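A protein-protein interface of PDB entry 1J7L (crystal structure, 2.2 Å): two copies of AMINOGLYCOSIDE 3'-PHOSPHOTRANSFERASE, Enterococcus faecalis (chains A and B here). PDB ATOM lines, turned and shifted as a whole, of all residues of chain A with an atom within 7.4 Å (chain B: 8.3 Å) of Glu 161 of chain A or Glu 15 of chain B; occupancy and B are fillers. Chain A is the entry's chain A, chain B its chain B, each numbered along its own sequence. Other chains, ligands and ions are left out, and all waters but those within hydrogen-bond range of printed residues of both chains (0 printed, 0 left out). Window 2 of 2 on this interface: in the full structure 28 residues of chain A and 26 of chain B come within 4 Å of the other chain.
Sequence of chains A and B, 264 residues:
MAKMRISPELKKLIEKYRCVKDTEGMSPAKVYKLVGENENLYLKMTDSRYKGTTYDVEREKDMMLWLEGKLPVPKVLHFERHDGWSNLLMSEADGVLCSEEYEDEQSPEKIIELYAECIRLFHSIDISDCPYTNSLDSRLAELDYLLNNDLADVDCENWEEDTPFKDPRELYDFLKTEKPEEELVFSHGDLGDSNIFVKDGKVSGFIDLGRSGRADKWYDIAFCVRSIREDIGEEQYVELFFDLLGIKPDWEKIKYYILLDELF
The side-chain amino group (NZ) of Lys 11 of chain B is in salt-bridge range of the side-chain carboxylate (OE2) of Glu 15 of chain B (2.9 Å).
The backbone carbonyl oxygen of Arg 18 of chain B lies within hydrogen-bond range of the backbone NH of Val 35 of chain B, at 2.8 Å.
The backbone NH (N) of Cys 19 of chain B lies within hydrogen-bond range of the side-chain carboxylate (OE2) of Glu 160 of chain A (3.2 Å).
The backbone NH of Glu 161 of chain A lies within hydrogen-bond range of the backbone carbonyl oxygen of Glu 15 of chain B (3.4 Å).
Trp 159 of chain A touches Ile 6 of chain B.
Trp 159 of chain A touches Lys 11 of chain B.
Tyr 17 of chain B touches Glu 160 of chain A (O to CG, 3.4 Å).
Arg 18 of chain B touches Glu 160 of chain A.
Glu 161 of chain A touches just one residue of chain B: Glu 15.
Of chain A, only Glu 161 (3.4 Å) comes within 4 Å of Glu 15 of chain B.
Of the printed residues of chain B, Glu 160 of chain A touches Tyr 17, Arg 18 and Cys 19.
Of the printed residues of chain A, Ile 6 of chain B touches Trp 159 (3.7 Å).
Printed residues of chain A within 4 Å of Cys 19 of chain B: Glu 160.
Printed residues of chain A within 4 Å of Tyr 17 of chain B: Glu 160 (3.4 Å).
The nearest residue of chain B that does not touch Glu 161 of chain A is Lys 16 of chain B (4.8 Å).
The nearest printed residue of chain B that does not touch Trp 159 of chain A is Ile 14 of chain B (4.04 Å).
Of the 9 printed residues of chain A, 3 touch a printed residue of chain B.
Printed residues of chain A that touch a printed residue of chain B: Trp 159, Glu 160 and Glu 161.
Of the 17 printed residues of chain B, 6 touch a printed residue of chain A.
Along chain B the printed residues that touch a printed residue of chain A span positions 6 to 19.
Among the printed residues, no Asp or Glu carboxylate lies within 4 Å of a Lys or Arg side-chain nitrogen of the other chain.
No position is printed for both chains.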
ATOM      1  N   GLU A 157     -36.149 -17.359  13.150  1.00  0.00           N
ATOM      2  CA  GLU A 157     -35.481 -16.129  13.566  1.00  0.00           C
ATOM      3  C   GLU A 157     -35.201 -16.184  15.072  1.00  0.00           C
ATOM      4  O   GLU A 157     -34.299 -15.511  15.571  1.00  0.00           O
ATOM      5  CB  GLU A 157     -36.353 -14.909  13.247  1.00  0.00           C
ATOM      6  CG  GLU A 157     -36.661 -14.718  11.761  1.00  0.00           C
ATOM      7  N   ASN A 158     -35.966 -17.008  15.784  1.00  0.00           N
ATOM      8  CA  ASN A 158     -35.800 -17.171  17.227  1.00  0.00           C
ATOM      9  C   ASN A 158     -34.482 -17.880  17.548  1.00  0.00           C
ATOM     10  O   ASN A 158     -34.082 -17.962  18.708  1.00  0.00           O
ATOM     11  CB  ASN A 158     -36.982 -17.950  17.819  1.00  0.00           C
ATOM     12  N   TRP A 159     -33.812 -18.399  16.522  1.00  0.00           N
ATOM     13  CA  TRP A 159     -32.533 -19.071  16.721  1.00  0.00           C
ATOM     14  C   TRP A 159     -31.385 -18.068  16.699  1.00  0.00           C
ATOM     15  O   TRP A 159     -30.282 -18.375  17.155  1.00  0.00           O
ATOM     16  CB  TRP A 159     -32.317 -20.160  15.669  1.00  0.00           C
ATOM     17  CG  TRP A 159     -33.193 -21.356  15.870  1.00  0.00           C
ATOM     18  CD1 TRP A 159     -33.697 -21.815  17.057  1.00  0.00           C
ATOM     19  CD2 TRP A 159     -33.673 -22.250  14.861  1.00  0.00           C
ATOM     20  NE1 TRP A 159     -34.460 -22.939  16.847  1.00  0.00           N
ATOM     21  CE2 TRP A 159     -34.463 -23.228  15.507  1.00  0.00           C
ATOM     22  CE3 TRP A 159     -33.513 -22.321  13.470  1.00  0.00           C
ATOM     23  CZ2 TRP A 159     -35.090 -24.262  14.812  1.00  0.00           C
ATOM     24  CZ3 TRP A 159     -34.137 -23.351  12.780  1.00  0.00           C
ATOM     25  CH2 TRP A 159     -34.917 -24.307  13.453  1.00  0.00           C
ATOM     26  N   GLU A 160     -31.657 -16.870  16.179  1.00  0.00           N
ATOM     27  CA  GLU A 160     -30.661 -15.800  16.103  1.00  0.00           C
ATOM     28  C   GLU A 160     -30.221 -15.388  17.511  1.00  0.00           C
ATOM     29  O   GLU A 160     -31.030 -15.357  18.436  1.00  0.00           O
ATOM     30  CB  GLU A 160     -31.227 -14.606  15.324  1.00  0.00           C
ATOM     31  CG  GLU A 160     -31.451 -14.902  13.836  1.00  0.00           C
ATOM     32  CD  GLU A 160     -32.242 -13.825  13.101  1.00  0.00           C
ATOM     33  OE1 GLU A 160     -32.178 -12.637  13.494  1.00  0.00           O
ATOM     34  OE2 GLU A 160     -32.926 -14.172  12.113  1.00  0.00           O
ATOM     35  N   GLU A 161     -28.935 -15.087  17.662  1.00  0.00           N
ATOM     36  CA  GLU A 161     -28.354 -14.718  18.953  1.00  0.00           C
ATOM     37  C   GLU A 161     -28.949 -13.509  19.688  1.00  0.00           C
ATOM     38  O   GLU A 161     -28.907 -13.453  20.920  1.00  0.00           O
ATOM     39  CB  GLU A 161     -26.840 -14.538  18.810  1.00  0.00           C
ATOM     40  CG  GLU A 161     -26.098 -14.373  20.137  1.00  0.00           C
ATOM     41  CD  GLU A 161     -24.590 -14.256  19.974  1.00  0.00           C
ATOM     42  OE1 GLU A 161     -24.108 -14.103  18.829  1.00  0.00           O
ATOM     43  OE2 GLU A 161     -23.881 -14.317  21.002  1.00  0.00           O
ATOM     44  N   ASP A 162     -29.508 -12.556  18.951  1.00  0.00           N
ATOM     45  CA  ASP A 162     -30.072 -11.359  19.572  1.00  0.00           C
ATOM     46  C   ASP A 162     -31.469 -11.516  20.185  1.00  0.00           C
ATOM     47  O   ASP A 162     -31.978 -10.589  20.818  1.00  0.00           O
ATOM     48  CB  ASP A 162     -30.039 -10.176  18.591  1.00  0.00           C
ATOM     49  CG  ASP A 162     -31.066 -10.297  17.471  1.00  0.00           C
ATOM     50  OD1 ASP A 162     -31.521 -11.422  17.165  1.00  0.00           O
ATOM     51  OD2 ASP A 162     -31.417  -9.248  16.888  1.00  0.00           O
ATOM     52  N   THR A 163     -32.085 -12.681  19.997  1.00  0.00           N
ATOM     53  CA  THR A 163     -33.419 -12.941  20.538  1.00  0.00           C
ATOM     54  C   THR A 163     -33.382 -12.989  22.067  1.00  0.00           C
ATOM     55  O   THR A 163     -32.516 -13.639  22.657  1.00  0.00           O
ATOM     56  CB  THR A 163     -34.014 -14.254  19.983  1.00  0.00           C
ATOM     57  N   PRO A 164     -34.324 -12.288  22.724  1.00  0.00           N
ATOM     58  CA  PRO A 164     -34.451 -12.204  24.185  1.00  0.00           C
ATOM     59  C   PRO A 164     -34.600 -13.554  24.877  1.00  0.00           C
ATOM     60  O   PRO A 164     -33.787 -13.919  25.729  1.00  0.00           O
ATOM     61  CB  PRO A 164     -35.704 -11.349  24.366  1.00  0.00           C
ATOM     62  CG  PRO A 164     -35.705 -10.484  23.145  1.00  0.00           C
ATOM     63  CD  PRO A 164     -35.373 -11.485  22.072  1.00  0.00           C
ATOM     64  N   LYS A 166     -34.339 -17.445  25.176  1.00  0.00           N
ATOM     65  CA  LYS A 166     -33.492 -18.507  24.635  1.00  0.00           C
ATOM     66  C   LYS A 166     -34.210 -19.767  24.147  1.00  0.00           C
ATOM     67  O   LYS A 166     -33.652 -20.532  23.362  1.00  0.00           O
ATOM     68  CB  LYS A 166     -32.383 -18.881  25.627  1.00  0.00           C
ATOM     69  CG  LYS A 166     -31.261 -17.846  25.745  1.00  0.00           C
ATOM     70  N   ILE B   6     -33.309 -28.069  17.721  1.00  0.00           N
ATOM     71  CA  ILE B   6     -31.878 -28.151  17.446  1.00  0.00           C
ATOM     72  C   ILE B   6     -31.114 -28.127  18.768  1.00  0.00           C
ATOM     73  O   ILE B   6     -31.569 -27.544  19.749  1.00  0.00           O
ATOM     74  CB  ILE B   6     -31.394 -27.006  16.519  1.00  0.00           C
ATOM     75  CG1 ILE B   6     -31.652 -25.639  17.157  1.00  0.00           C
ATOM     76  CG2 ILE B   6     -32.088 -27.102  15.156  1.00  0.00           C
ATOM     77  CD1 ILE B   6     -31.070 -24.472  16.362  1.00  0.00           C
ATOM     78  N   PRO B   8     -27.958 -27.379  21.536  1.00  0.00           N
ATOM     79  CA  PRO B   8     -27.264 -26.132  21.852  1.00  0.00           C
ATOM     80  C   PRO B   8     -26.011 -25.940  20.990  1.00  0.00           C
ATOM     81  O   PRO B   8     -25.690 -24.812  20.631  1.00  0.00           O
ATOM     82  CB  PRO B   8     -26.958 -26.266  23.353  1.00  0.00           C
ATOM     83  CG  PRO B   8     -27.137 -27.724  23.654  1.00  0.00           C
ATOM     84  CD  PRO B   8     -28.251 -28.141  22.761  1.00  0.00           C
ATOM     85  N   GLU B   9     -25.364 -27.040  20.592  1.00  0.00           N
ATOM     86  CA  GLU B   9     -24.163 -26.975  19.740  1.00  0.00           C
ATOM     87  C   GLU B   9     -24.509 -26.427  18.372  1.00  0.00           C
ATOM     88  O   GLU B   9     -23.776 -25.604  17.826  1.00  0.00           O
ATOM     89  CB  GLU B   9     -23.543 -28.349  19.511  1.00  0.00           C
ATOM     90  CG  GLU B   9     -23.499 -29.226  20.707  1.00  0.00           C
ATOM     91  CD  GLU B   9     -24.717 -30.108  20.834  1.00  0.00           C
ATOM     92  OE1 GLU B   9     -24.789 -31.127  20.118  1.00  0.00           O
ATOM     93  OE2 GLU B   9     -25.588 -29.790  21.660  1.00  0.00           O
ATOM     94  N   LEU B  10     -25.589 -26.945  17.790  1.00  0.00           N
ATOM     95  CA  LEU B  10     -26.036 -26.491  16.479  1.00  0.00           C
ATOM     96  C   LEU B  10     -26.508 -25.053  16.578  1.00  0.00           C
ATOM     97  O   LEU B  10     -26.187 -24.226  15.728  1.00  0.00           O
ATOM     98  CB  LEU B  10     -27.161 -27.372  15.950  1.00  0.00           C
ATOM     99  CG  LEU B  10     -27.734 -26.986  14.581  1.00  0.00           C
ATOM    100  CD1 LEU B  10     -26.611 -26.747  13.577  1.00  0.00           C
ATOM    101  CD2 LEU B  10     -28.670 -28.084  14.091  1.00  0.00           C
ATOM    102  N   LYS B  11     -27.264 -24.757  17.629  1.00  0.00           N
ATOM    103  CA  LYS B  11     -27.768 -23.409  17.861  1.00  0.00           C
ATOM    104  C   LYS B  11     -26.582 -22.441  17.915  1.00  0.00           C
ATOM    105  O   LYS B  11     -26.609 -21.375  17.303  1.00  0.00           O
ATOM    106  CB  LYS B  11     -28.555 -23.365  19.174  1.00  0.00           C
ATOM    107  CG  LYS B  11     -29.450 -22.151  19.333  1.00  0.00           C
ATOM    108  CD  LYS B  11     -28.939 -21.230  20.417  1.00  0.00           C
ATOM    109  CE  LYS B  11     -29.800 -19.978  20.511  1.00  0.00           C
ATOM    110  NZ  LYS B  11     -29.176 -18.960  21.395  1.00  0.00           N
ATOM    111  N   LYS B  12     -25.521 -22.860  18.597  1.00  0.00           N
ATOM    112  CA  LYS B  12     -24.307 -22.059  18.741  1.00  0.00           C
ATOM    113  C   LYS B  12     -23.647 -21.801  17.385  1.00  0.00           C
ATOM    114  O   LYS B  12     -23.152 -20.701  17.126  1.00  0.00           O
ATOM    115  CB  LYS B  12     -23.311 -22.779  19.654  1.00  0.00           C
ATOM    116  CG  LYS B  12     -22.137 -21.923  20.109  1.00  0.00           C
ATOM    117  CD  LYS B  12     -22.583 -20.920  21.161  1.00  0.00           C
ATOM    118  CE  LYS B  12     -21.412 -20.149  21.746  1.00  0.00           C
ATOM    119  NZ  LYS B  12     -21.857 -19.308  22.898  1.00  0.00           N
ATOM    120  N   LEU B  13     -23.655 -22.819  16.527  1.00  0.00           N
ATOM    121  CA  LEU B  13     -23.054 -22.733  15.198  1.00  0.00           C
ATOM    122  C   LEU B  13     -23.763 -21.776  14.251  1.00  0.00           C
ATOM    123  O   LEU B  13     -23.127 -21.169  13.387  1.00  0.00           O
ATOM    124  CB  LEU B  13     -22.992 -24.120  14.558  1.00  0.00           C
ATOM    125  CG  LEU B  13     -21.980 -25.078  15.181  1.00  0.00           C
ATOM    126  CD1 LEU B  13     -22.262 -26.497  14.730  1.00  0.00           C
ATOM    127  CD2 LEU B  13     -20.561 -24.640  14.812  1.00  0.00           C
ATOM    128  N   ILE B  14     -25.075 -21.635  14.418  1.00  0.00           N
ATOM    129  CA  ILE B  14     -25.858 -20.764  13.549  1.00  0.00           C
ATOM    130  C   ILE B  14     -26.287 -19.428  14.168  1.00  0.00           C
ATOM    131  O   ILE B  14     -26.987 -18.648  13.521  1.00  0.00           O
ATOM    132  CB  ILE B  14     -27.113 -21.494  13.015  1.00  0.00           C
ATOM    133  CG1 ILE B  14     -28.150 -21.670  14.129  1.00  0.00           C
ATOM    134  CG2 ILE B  14     -26.718 -22.858  12.448  1.00  0.00           C
ATOM    135  CD1 ILE B  14     -29.477 -22.218  13.654  1.00  0.00           C
ATOM    136  N   GLU B  15     -25.860 -19.167  15.403  1.00  0.00           N
ATOM    137  CA  GLU B  15     -26.215 -17.930  16.111  1.00  0.00           C
ATOM    138  C   GLU B  15     -25.872 -16.662  15.336  1.00  0.00           C
ATOM    139  O   GLU B  15     -26.692 -15.744  15.231  1.00  0.00           O
ATOM    140  CB  GLU B  15     -25.524 -17.869  17.477  1.00  0.00           C
ATOM    141  CG  GLU B  15     -26.253 -18.591  18.592  1.00  0.00           C
ATOM    142  CD  GLU B  15     -25.596 -18.400  19.951  1.00  0.00           C
ATOM    143  OE1 GLU B  15     -24.398 -18.036  20.012  1.00  0.00           O
ATOM    144  OE2 GLU B  15     -26.286 -18.625  20.966  1.00  0.00           O
ATOM    145  N   LYS B  16     -24.651 -16.628  14.813  1.00  0.00           N
ATOM    146  CA  LYS B  16     -24.134 -15.503  14.042  1.00  0.00           C
ATOM    147  C   LYS B  16     -24.898 -15.269  12.734  1.00  0.00           C
ATOM    148  O   LYS B  16     -24.774 -14.207  12.114  1.00  0.00           O
ATOM    149  CB  LYS B  16     -22.656 -15.756  13.736  1.00  0.00           C
ATOM    150  N   TYR B  17     -25.700 -16.248  12.327  1.00  0.00           N
ATOM    151  CA  TYR B  17     -26.449 -16.139  11.083  1.00  0.00           C
ATOM    152  C   TYR B  17     -27.860 -15.602  11.229  1.00  0.00           C
ATOM    153  O   TYR B  17     -28.490 -15.731  12.274  1.00  0.00           O
ATOM    154  CB  TYR B  17     -26.482 -17.489  10.356  1.00  0.00           C
ATOM    155  CG  TYR B  17     -25.116 -18.008   9.982  1.00  0.00           C
ATOM    156  CD1 TYR B  17     -24.377 -18.782  10.875  1.00  0.00           C
ATOM    157  CD2 TYR B  17     -24.552 -17.714   8.744  1.00  0.00           C
ATOM    158  CE1 TYR B  17     -23.109 -19.248  10.546  1.00  0.00           C
ATOM    159  CE2 TYR B  17     -23.280 -18.177   8.404  1.00  0.00           C
ATOM    160  CZ  TYR B  17     -22.569 -18.942   9.309  1.00  0.00           C
ATOM    161  OH  TYR B  17     -21.320 -19.416   8.978  1.00  0.00           O
ATOM    162  N   ARG B  18     -28.326 -14.968  10.162  1.00  0.00           N
ATOM    163  CA  ARG B  18     -29.665 -14.406  10.100  1.00  0.00           C
ATOM    164  C   ARG B  18     -30.475 -15.410   9.283  1.00  0.00           C
ATOM    165  O   ARG B  18     -30.163 -15.672   8.120  1.00  0.00           O
ATOM    166  CB  ARG B  18     -29.610 -13.033   9.418  1.00  0.00           C
ATOM    167  CG  ARG B  18     -30.939 -12.315   9.258  1.00  0.00           C
ATOM    168  CD  ARG B  18     -31.713 -12.832   8.056  1.00  0.00           C
ATOM    169  NE  ARG B  18     -32.857 -11.990   7.724  1.00  0.00           N
ATOM    170  CZ  ARG B  18     -32.991 -11.338   6.572  1.00  0.00           C
ATOM    171  NH1 ARG B  18     -32.047 -11.436   5.639  1.00  0.00           N
ATOM    172  NH2 ARG B  18     -34.064 -10.584   6.357  1.00  0.00           N
ATOM    173  N   CYS B  19     -31.500 -15.987   9.901  1.00  0.00           N
ATOM    174  CA  CYS B  19     -32.322 -16.983   9.228  1.00  0.00           C
ATOM    175  C   CYS B  19     -33.366 -16.472   8.253  1.00  0.00           C
ATOM    176  O   CYS B  19     -34.077 -15.510   8.527  1.00  0.00           O
ATOM    177  CB  CYS B  19     -33.012 -17.901  10.233  1.00  0.00           C
ATOM    178  SG  CYS B  19     -33.996 -19.170   9.377  1.00  0.00           S
ATOM    179  N   LEU B  34     -29.314 -19.544   6.000  1.00  0.00           N
ATOM    180  CA  LEU B  34     -28.685 -18.815   7.088  1.00  0.00           C
ATOM    181  C   LEU B  34     -27.704 -17.815   6.490  1.00  0.00           C
ATOM    182  O   LEU B  34     -26.589 -18.176   6.112  1.00  0.00           O
ATOM    183  CB  LEU B  34     -27.974 -19.790   8.028  1.00  0.00           C
ATOM    184  CG  LEU B  34     -28.862 -20.898   8.608  1.00  0.00           C
ATOM    185  CD1 LEU B  34     -28.001 -21.901   9.352  1.00  0.00           C
ATOM    186  CD2 LEU B  34     -29.925 -20.319   9.523  1.00  0.00           C
ATOM    187  N   VAL B  35     -28.154 -16.569   6.364  1.00  0.00           N
ATOM    188  CA  VAL B  35     -27.340 -15.501   5.792  1.00  0.00           C
ATOM    189  C   VAL B  35     -26.315 -14.960   6.782  1.00  0.00           C
ATOM    190  O   VAL B  35     -26.661 -14.517   7.873  1.00  0.00           O
ATOM    191  CB  VAL B  35     -28.212 -14.334   5.265  1.00  0.00           C
ATOM    192  CG1 VAL B  35     -27.340 -13.270   4.614  1.00  0.00           C
ATOM    193  CG2 VAL B  35     -29.240 -14.856   4.262  1.00  0.00           C
ATOM    194  N   LEU B  41     -25.253 -20.419   4.815  1.00  0.00           N
ATOM    195  CA  LEU B  41     -25.328 -21.841   5.079  1.00  0.00           C
ATOM    196  C   LEU B  41     -26.782 -22.231   4.908  1.00  0.00           C
ATOM    197  O   LEU B  41     -27.646 -21.376   4.713  1.00  0.00           O
ATOM    198  CB  LEU B  41     -24.859 -22.168   6.500  1.00  0.00           C
ATOM    199  CG  LEU B  41     -23.485 -21.633   6.934  1.00  0.00           C
ATOM    200  CD1 LEU B  41     -23.130 -22.179   8.317  1.00  0.00           C
ATOM    201  CD2 LEU B  41     -22.416 -22.016   5.921  1.00  0.00           C
ATOM    202  N   LEU B  89     -26.639 -29.147   8.666  1.00  0.00           N
ATOM    203  CA  LEU B  89     -26.116 -27.818   8.378  1.00  0.00           C
ATOM    204  C   LEU B  89     -25.123 -28.069   7.248  1.00  0.00           C
ATOM    205  O   LEU B  89     -24.216 -28.896   7.386  1.00  0.00           O
ATOM    206  CB  LEU B  89     -25.396 -27.236   9.603  1.00  0.00           C
ATOM    207  CG  LEU B  89     -24.910 -25.787   9.477  1.00  0.00           C
ATOM    208  CD1 LEU B  89     -26.108 -24.867   9.327  1.00  0.00           C
ATOM    209  CD2 LEU B  89     -24.069 -25.387  10.698  1.00  0.00           C
